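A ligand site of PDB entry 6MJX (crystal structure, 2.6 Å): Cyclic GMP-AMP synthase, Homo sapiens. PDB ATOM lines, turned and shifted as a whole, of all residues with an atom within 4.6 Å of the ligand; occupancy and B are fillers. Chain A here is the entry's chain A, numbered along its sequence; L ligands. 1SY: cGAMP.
The backbone NH of Arg 226 lies within hydrogen-bond range of the backbone carbonyl oxygen of Lys 212 (3.3 Å).
The backbone carbonyl oxygen of Arg 226 lies within hydrogen-bond range of the backbone NH of Val 210 (2.8 Å).
The side-chain hydroxyl of Ser 284 sits close to the backbone NH of Tyr 286, 3.1 Å away.
The backbone NH (N) of Ser 284 sits at hydrogen-bond distance from a ring nitrogen (ND1) of His 287 (2.9 Å).
The side-chain carboxylate (OE2) of Glu 233 is in hydrogen-bond range of the side-chain hydroxyl (OH) of Tyr 286 (2.8 Å).
The side-chain carboxylate (OD1) of Asp 77 sits at hydrogen-bond distance from a nitrogen (N41) of the ligand (2.7 Å).
NZ of Lys 212 lies within salt-bridge range of O30 of the ligand (2.8 Å).
A nitrogen (N35) of the ligand lies within hydrogen-bond range of the guanidinium group (NH2) of Arg 226 (2.9 Å).
A nitrogen (N41) of the ligand sits at hydrogen-bond distance from the side-chain carboxylate (OD2) of Asp 169 (3.1 Å).
An oxygen (O19) of the ligand sits close to the side-chain hydroxyl of Ser 284 (3.4 Å).
N1 of the ligand sits close to OH of Tyr 286, 3.3 Å away.
Lys 151 touches the ligand (NZ to O23, 3.9 Å).
Gly 154 touches the ligand.
Ser 155 touches the ligand.
CD of Pro 156 touches C36 of the ligand (3.6 Å).
Ala 157 touches the ligand (CB to N41, 3.9 Å).
Thr 171 touches the ligand (OG1 to N41, 3.8 Å).
Of the 21 residues printed, 12 come within 4 Å of the ligand.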
ATOM      1  N   ASP A  77      -9.077   1.185  25.812  1.00  0.00           N
ATOM      2  CA  ASP A  77      -9.179  -0.237  25.470  1.00  0.00           C
ATOM      3  C   ASP A  77      -7.781  -0.844  25.498  1.00  0.00           C
ATOM      4  O   ASP A  77      -6.942  -0.532  24.640  1.00  0.00           O
ATOM      5  CB  ASP A  77      -9.838  -0.434  24.105  1.00  0.00           C
ATOM      6  CG  ASP A  77     -10.270  -1.872  23.878  1.00  0.00           C
ATOM      7  OD1 ASP A  77     -10.742  -2.514  24.848  1.00  0.00           O
ATOM      8  OD2 ASP A  77     -10.134  -2.365  22.738  1.00  0.00           O
ATOM      9  N   TYR A  98     -17.056 -16.841  16.032  1.00  0.00           N
ATOM     10  CA  TYR A  98     -16.950 -17.417  17.363  1.00  0.00           C
ATOM     11  C   TYR A  98     -16.410 -18.852  17.266  1.00  0.00           C
ATOM     12  O   TYR A  98     -16.761 -19.592  16.337  1.00  0.00           O
ATOM     13  CB  TYR A  98     -18.288 -17.391  18.095  1.00  0.00           C
ATOM     14  CG  TYR A  98     -18.841 -15.995  18.292  1.00  0.00           C
ATOM     15  CD1 TYR A  98     -19.676 -15.413  17.344  1.00  0.00           C
ATOM     16  CD2 TYR A  98     -18.508 -15.245  19.413  1.00  0.00           C
ATOM     17  CE1 TYR A  98     -20.174 -14.146  17.508  1.00  0.00           C
ATOM     18  CE2 TYR A  98     -19.001 -13.962  19.577  1.00  0.00           C
ATOM     19  CZ  TYR A  98     -19.831 -13.422  18.627  1.00  0.00           C
ATOM     20  OH  TYR A  98     -20.332 -12.149  18.785  1.00  0.00           O
ATOM     21  N   LYS A 151     -20.021  -4.954  32.535  1.00  0.00           N
ATOM     22  CA  LYS A 151     -20.638  -4.355  31.356  1.00  0.00           C
ATOM     23  C   LYS A 151     -21.742  -5.256  30.831  1.00  0.00           C
ATOM     24  O   LYS A 151     -21.920  -6.400  31.262  1.00  0.00           O
ATOM     25  CB  LYS A 151     -19.577  -4.093  30.288  1.00  0.00           C
ATOM     26  CG  LYS A 151     -19.923  -2.976  29.324  1.00  0.00           C
ATOM     27  CD  LYS A 151     -20.292  -1.704  30.069  1.00  0.00           C
ATOM     28  CE  LYS A 151     -20.319  -0.526  29.111  1.00  0.00           C
ATOM     29  NZ  LYS A 151     -21.130  -0.843  27.907  1.00  0.00           N
ATOM     30  N   ARG A 152     -22.497  -4.720  29.864  1.00  0.00           N
ATOM     31  CA  ARG A 152     -23.668  -5.404  29.331  1.00  0.00           C
ATOM     32  C   ARG A 152     -23.311  -6.817  28.875  1.00  0.00           C
ATOM     33  O   ARG A 152     -22.189  -7.095  28.447  1.00  0.00           O
ATOM     34  CB  ARG A 152     -24.273  -4.598  28.176  1.00  0.00           C
ATOM     35  CG  ARG A 152     -24.430  -3.110  28.468  1.00  0.00           C
ATOM     36  CD  ARG A 152     -25.197  -2.884  29.770  1.00  0.00           C
ATOM     37  NE  ARG A 152     -25.227  -1.473  30.154  1.00  0.00           N
ATOM     38  CZ  ARG A 152     -26.259  -0.662  29.962  1.00  0.00           C
ATOM     39  NH1 ARG A 152     -26.196   0.609  30.346  1.00  0.00           N
ATOM     40  NH2 ARG A 152     -27.358  -1.109  29.372  1.00  0.00           N
ATOM     41  N   GLY A 153     -24.292  -7.717  28.973  1.00  0.00           N
ATOM     42  CA  GLY A 153     -24.105  -9.136  28.709  1.00  0.00           C
ATOM     43  C   GLY A 153     -23.329  -9.473  27.455  1.00  0.00           C
ATOM     44  O   GLY A 153     -23.767  -9.187  26.334  1.00  0.00           O
ATOM     45  N   GLY A 154     -22.169 -10.079  27.637  1.00  0.00           N
ATOM     46  CA  GLY A 154     -21.311 -10.504  26.540  1.00  0.00           C
ATOM     47  C   GLY A 154     -19.985  -9.790  26.471  1.00  0.00           C
ATOM     48  O   GLY A 154     -19.124 -10.216  25.678  1.00  0.00           O
ATOM     49  N   SER A 155     -19.758  -8.752  27.261  1.00  0.00           N
ATOM     50  CA  SER A 155     -18.526  -7.987  27.162  1.00  0.00           C
ATOM     51  C   SER A 155     -17.344  -8.834  27.594  1.00  0.00           C
ATOM     52  O   SER A 155     -17.300  -9.292  28.746  1.00  0.00           O
ATOM     53  CB  SER A 155     -18.608  -6.730  28.027  1.00  0.00           C
ATOM     54  OG  SER A 155     -17.417  -5.972  27.909  1.00  0.00           O
ATOM     55  N   PRO A 156     -16.360  -9.079  26.713  1.00  0.00           N
ATOM     56  CA  PRO A 156     -15.204  -9.889  27.090  1.00  0.00           C
ATOM     57  C   PRO A 156     -14.216  -9.153  27.965  1.00  0.00           C
ATOM     58  O   PRO A 156     -13.232  -9.771  28.410  1.00  0.00           O
ATOM     59  CB  PRO A 156     -14.576 -10.237  25.736  1.00  0.00           C
ATOM     60  CG  PRO A 156     -14.839  -9.005  24.925  1.00  0.00           C
ATOM     61  CD  PRO A 156     -16.209  -8.508  25.361  1.00  0.00           C
ATOM     62  N   ALA A 157     -14.429  -7.871  28.221  1.00  0.00           N
ATOM     63  CA  ALA A 157     -13.459  -7.052  28.908  1.00  0.00           C
ATOM     64  C   ALA A 157     -13.710  -7.025  30.408  1.00  0.00           C
ATOM     65  O   ALA A 157     -14.727  -7.508  30.918  1.00  0.00           O
ATOM     66  CB  ALA A 157     -13.457  -5.637  28.348  1.00  0.00           C
ATOM     67  N   ASP A 169     -10.793  -0.335  29.768  1.00  0.00           N
ATOM     68  CA  ASP A 169     -11.229  -1.663  29.374  1.00  0.00           C
ATOM     69  C   ASP A 169     -10.006  -2.569  29.278  1.00  0.00           C
ATOM     70  O   ASP A 169      -9.043  -2.257  28.577  1.00  0.00           O
ATOM     71  CB  ASP A 169     -11.984  -1.648  28.038  1.00  0.00           C
ATOM     72  CG  ASP A 169     -13.436  -1.224  28.187  1.00  0.00           C
ATOM     73  OD1 ASP A 169     -13.697  -0.252  28.929  1.00  0.00           O
ATOM     74  OD2 ASP A 169     -14.308  -1.866  27.562  1.00  0.00           O
ATOM     75  N   THR A 171      -9.103  -6.461  28.361  1.00  0.00           N
ATOM     76  CA  THR A 171      -9.599  -7.676  27.752  1.00  0.00           C
ATOM     77  C   THR A 171      -8.476  -8.710  27.730  1.00  0.00           C
ATOM     78  O   THR A 171      -7.350  -8.401  27.325  1.00  0.00           O
ATOM     79  CB  THR A 171     -10.095  -7.416  26.322  1.00  0.00           C
ATOM     80  OG1 THR A 171     -10.753  -6.146  26.260  1.00  0.00           O
ATOM     81  CG2 THR A 171     -11.073  -8.508  25.893  1.00  0.00           C
ATOM     82  N   VAL A 210     -10.895 -13.398  22.130  1.00  0.00           N
ATOM     83  CA  VAL A 210     -11.304 -12.728  23.364  1.00  0.00           C
ATOM     84  C   VAL A 210     -12.498 -13.479  23.942  1.00  0.00           C
ATOM     85  O   VAL A 210     -13.294 -14.053  23.180  1.00  0.00           O
ATOM     86  CB  VAL A 210     -11.644 -11.241  23.112  1.00  0.00           C
ATOM     87  CG1 VAL A 210     -10.438 -10.523  22.539  1.00  0.00           C
ATOM     88  CG2 VAL A 210     -12.845 -11.120  22.175  1.00  0.00           C
ATOM     89  N   LYS A 212     -15.415 -13.226  24.430  1.00  0.00           N
ATOM     90  CA  LYS A 212     -16.762 -12.807  24.036  1.00  0.00           C
ATOM     91  C   LYS A 212     -17.491 -14.041  23.530  1.00  0.00           C
ATOM     92  O   LYS A 212     -17.020 -14.730  22.618  1.00  0.00           O
ATOM     93  CB  LYS A 212     -16.681 -11.707  22.972  1.00  0.00           C
ATOM     94  CG  LYS A 212     -17.866 -11.632  22.012  1.00  0.00           C
ATOM     95  CD  LYS A 212     -19.168 -11.178  22.671  1.00  0.00           C
ATOM     96  CE  LYS A 212     -20.351 -11.350  21.700  1.00  0.00           C
ATOM     97  NZ  LYS A 212     -21.683 -11.055  22.302  1.00  0.00           N
ATOM     98  N   ARG A 226     -14.365 -15.147  20.625  1.00  0.00           N
ATOM     99  CA  ARG A 226     -14.510 -14.452  19.354  1.00  0.00           C
ATOM    100  C   ARG A 226     -13.143 -13.964  18.869  1.00  0.00           C
ATOM    101  O   ARG A 226     -12.301 -13.548  19.662  1.00  0.00           O
ATOM    102  CB  ARG A 226     -15.467 -13.248  19.448  1.00  0.00           C
ATOM    103  CG  ARG A 226     -15.632 -12.535  18.114  1.00  0.00           C
ATOM    104  CD  ARG A 226     -16.617 -11.384  18.124  1.00  0.00           C
ATOM    105  NE  ARG A 226     -16.417 -10.440  19.211  1.00  0.00           N
ATOM    106  CZ  ARG A 226     -15.347  -9.666  19.375  1.00  0.00           C
ATOM    107  NH1 ARG A 226     -14.334  -9.721  18.524  1.00  0.00           N
ATOM    108  NH2 ARG A 226     -15.304  -8.828  20.405  1.00  0.00           N
ATOM    109  N   SER A 228     -10.394 -11.513  17.205  1.00  0.00           N
ATOM    110  CA  SER A 228     -10.116 -10.098  17.368  1.00  0.00           C
ATOM    111  C   SER A 228      -8.896  -9.749  16.527  1.00  0.00           C
ATOM    112  O   SER A 228      -7.858 -10.412  16.629  1.00  0.00           O
ATOM    113  CB  SER A 228      -9.875  -9.729  18.835  1.00  0.00           C
ATOM    114  OG  SER A 228      -9.589  -8.341  18.983  1.00  0.00           O
ATOM    115  N   GLU A 233      -6.296  -3.579  13.163  1.00  0.00           N
ATOM    116  CA  GLU A 233      -7.123  -2.388  12.988  1.00  0.00           C
ATOM    117  C   GLU A 233      -6.331  -1.117  13.272  1.00  0.00           C
ATOM    118  O   GLU A 233      -6.464  -0.120  12.557  1.00  0.00           O
ATOM    119  CB  GLU A 233      -8.355  -2.457  13.876  1.00  0.00           C
ATOM    120  CG  GLU A 233      -9.336  -3.537  13.491  1.00  0.00           C
ATOM    121  CD  GLU A 233     -10.409  -3.766  14.553  1.00  0.00           C
ATOM    122  OE1 GLU A 233     -10.399  -3.044  15.569  1.00  0.00           O
ATOM    123  OE2 GLU A 233     -11.241  -4.671  14.368  1.00  0.00           O
ATOM    124  N   LYS A 282     -27.577  -0.625  20.618  1.00  0.00           N
ATOM    125  CA  LYS A 282     -26.807  -1.649  19.913  1.00  0.00           C
ATOM    126  C   LYS A 282     -25.705  -1.064  19.032  1.00  0.00           C
ATOM    127  O   LYS A 282     -24.768  -1.793  18.698  1.00  0.00           O
ATOM    128  CB  LYS A 282     -27.751  -2.505  19.048  1.00  0.00           C
ATOM    129  CG  LYS A 282     -28.867  -3.183  19.815  1.00  0.00           C
ATOM    130  CD  LYS A 282     -28.338  -4.082  20.922  1.00  0.00           C
ATOM    131  CE  LYS A 282     -29.478  -4.788  21.627  1.00  0.00           C
ATOM    132  NZ  LYS A 282     -29.015  -5.519  22.839  1.00  0.00           N
ATOM    133  N   SER A 284     -22.414   0.918  18.120  1.00  0.00           N
ATOM    134  CA  SER A 284     -21.194   1.361  18.774  1.00  0.00           C
ATOM    135  C   SER A 284     -20.229   1.955  17.751  1.00  0.00           C
ATOM    136  O   SER A 284     -20.430   1.863  16.542  1.00  0.00           O
ATOM    137  CB  SER A 284     -20.505   0.208  19.523  1.00  0.00           C
ATOM    138  OG  SER A 284     -19.725  -0.567  18.637  1.00  0.00           O
ATOM    139  N   TYR A 286     -17.472   0.836  16.982  1.00  0.00           N
ATOM    140  CA  TYR A 286     -16.880  -0.210  16.151  1.00  0.00           C
ATOM    141  C   TYR A 286     -17.640  -0.386  14.848  1.00  0.00           C
ATOM    142  O   TYR A 286     -17.039  -0.709  13.808  1.00  0.00           O
ATOM    143  CB  TYR A 286     -16.822  -1.529  16.914  1.00  0.00           C
ATOM    144  CG  TYR A 286     -16.047  -2.596  16.195  1.00  0.00           C
ATOM    145  CD1 TYR A 286     -14.654  -2.597  16.211  1.00  0.00           C
ATOM    146  CD2 TYR A 286     -16.704  -3.611  15.497  1.00  0.00           C
ATOM    147  CE1 TYR A 286     -13.937  -3.582  15.566  1.00  0.00           C
ATOM    148  CE2 TYR A 286     -15.988  -4.596  14.838  1.00  0.00           C
ATOM    149  CZ  TYR A 286     -14.601  -4.577  14.876  1.00  0.00           C
ATOM    150  OH  TYR A 286     -13.889  -5.549  14.231  1.00  0.00           O
ATOM    151  N   HIS A 287     -18.966  -0.212  14.859  1.00  0.00           N
ATOM    152  CA  HIS A 287     -19.724  -0.179  13.616  1.00  0.00           C
ATOM    153  C   HIS A 287     -19.233   0.956  12.730  1.00  0.00           C
ATOM    154  O   HIS A 287     -19.018   0.771  11.528  1.00  0.00           O
ATOM    155  CB  HIS A 287     -21.226  -0.016  13.891  1.00  0.00           C
ATOM    156  CG  HIS A 287     -21.845  -1.133  14.669  1.00  0.00           C
ATOM    157  ND1 HIS A 287     -22.397  -0.949  15.917  1.00  0.00           N
ATOM    158  CD2 HIS A 287     -22.028  -2.442  14.369  1.00  0.00           C
ATOM    159  CE1 HIS A 287     -22.880  -2.104  16.356  1.00  0.00           C
ATOM    160  NE2 HIS A 287     -22.667  -3.020  15.439  1.00  0.00           N
ATOM    161  N   ASN A 332     -18.164  -7.583   8.776  1.00  0.00           N
ATOM    162  CA  ASN A 332     -16.913  -7.455   9.502  1.00  0.00           C
ATOM    163  C   ASN A 332     -15.764  -7.374   8.498  1.00  0.00           C
ATOM    164  O   ASN A 332     -15.723  -8.115   7.515  1.00  0.00           O
ATOM    165  CB  ASN A 332     -16.733  -8.645  10.445  1.00  0.00           C
ATOM    166  CG  ASN A 332     -15.490  -8.539  11.299  1.00  0.00           C
ATOM    167  OD1 ASN A 332     -14.366  -8.739  10.816  1.00  0.00           O
ATOM    168  ND2 ASN A 332     -15.669  -8.238  12.573  1.00  0.00           N
HETATM  169  C2  1SY L   1     -15.089  -7.421  16.656  1.00  0.00           C
HETATM  170  N01 1SY L   1     -12.875  -5.460  18.650  1.00  0.00           N
HETATM  171  C6  1SY L   1     -14.166  -5.895  18.148  1.00  0.00           C
HETATM  172  N1  1SY L   1     -14.016  -6.871  17.255  1.00  0.00           N
HETATM  173  N3  1SY L   1     -16.333  -6.996  16.971  1.00  0.00           N
HETATM  174  C4  1SY L   1     -16.496  -6.009  17.879  1.00  0.00           C
HETATM  175  C5  1SY L   1     -15.433  -5.463  18.465  1.00  0.00           C
HETATM  176  N7  1SY L   1     -15.864  -4.509  19.315  1.00  0.00           N
HETATM  177  C8  1SY L   1     -17.205  -4.481  19.247  1.00  0.00           C
HETATM  178  N9  1SY L   1     -17.595  -5.402  18.361  1.00  0.00           N
HETATM  179  C1' 1SY L   1     -18.961  -5.637  18.028  1.00  0.00           C
HETATM  180  C2' 1SY L   1     -19.554  -6.623  18.999  1.00  0.00           C
HETATM  181  O2' 1SY L   1     -20.136  -7.701  18.282  1.00  0.00           O
HETATM  182  C3' 1SY L   1     -20.565  -5.897  19.796  1.00  0.00           C
HETATM  183  C4' 1SY L   1     -20.792  -4.634  19.089  1.00  0.00           C
HETATM  184  C16 1SY L   1     -20.820  -3.452  20.079  1.00  0.00           C
HETATM  185  O17 1SY L   1     -19.566  -3.366  20.775  1.00  0.00           O
HETATM  186  P18 1SY L   1     -19.354  -2.228  22.035  1.00  0.00           P
HETATM  187  O19 1SY L   1     -18.401  -1.097  21.707  1.00  0.00           O
HETATM  188  O20 1SY L   1     -19.082  -2.923  23.534  1.00  0.00           O
HETATM  189  C21 1SY L   1     -19.587  -4.311  23.488  1.00  0.00           C
HETATM  190  C22 1SY L   1     -20.937  -4.449  24.049  1.00  0.00           C
HETATM  191  O23 1SY L   1     -21.191  -3.491  25.081  1.00  0.00           O
HETATM  192  C24 1SY L   1     -20.986  -5.845  24.646  1.00  0.00           C
HETATM  193  C25 1SY L   1     -21.729  -6.781  23.826  1.00  0.00           C
HETATM  194  O26 1SY L   1     -21.900  -6.294  22.461  1.00  0.00           O
HETATM  195  P27 1SY L   1     -21.857  -7.564  21.336  1.00  0.00           P
HETATM  196  O28 1SY L   1     -21.797  -6.692  19.880  1.00  0.00           O
HETATM  197  O29 1SY L   1     -20.520  -8.250  21.514  1.00  0.00           O
HETATM  198  O30 1SY L   1     -22.903  -8.638  21.464  1.00  0.00           O
HETATM  199  O31 1SY L   1     -19.570  -6.289  24.725  1.00  0.00           O
HETATM  200  C32 1SY L   1     -18.777  -5.138  24.307  1.00  0.00           C
HETATM  201  N33 1SY L   1     -17.617  -5.624  23.541  1.00  0.00           N
HETATM  202  C34 1SY L   1     -17.850  -6.547  22.590  1.00  0.00           C
HETATM  203  N35 1SY L   1     -16.661  -6.879  22.038  1.00  0.00           N
HETATM  204  C36 1SY L   1     -16.306  -5.391  23.586  1.00  0.00           C
HETATM  205  C37 1SY L   1     -15.711  -6.163  22.646  1.00  0.00           C
HETATM  206  C38 1SY L   1     -14.191  -6.097  22.458  1.00  0.00           C
HETATM  207  N39 1SY L   1     -13.407  -5.214  23.282  1.00  0.00           N
HETATM  208  C40 1SY L   1     -14.057  -4.403  24.268  1.00  0.00           C
HETATM  209  N41 1SY L   1     -13.277  -3.507  25.107  1.00  0.00           N
HETATM  210  N42 1SY L   1     -15.504  -4.466  24.445  1.00  0.00           N
HETATM  211  O43 1SY L   1     -13.656  -6.773  21.636  1.00  0.00           O
HETATM  212  O44 1SY L   1     -20.707  -1.573  22.197  1.00  0.00           O
HETATM  213  O4' 1SY L   1     -19.713  -4.413  18.119  1.00  0.00           O
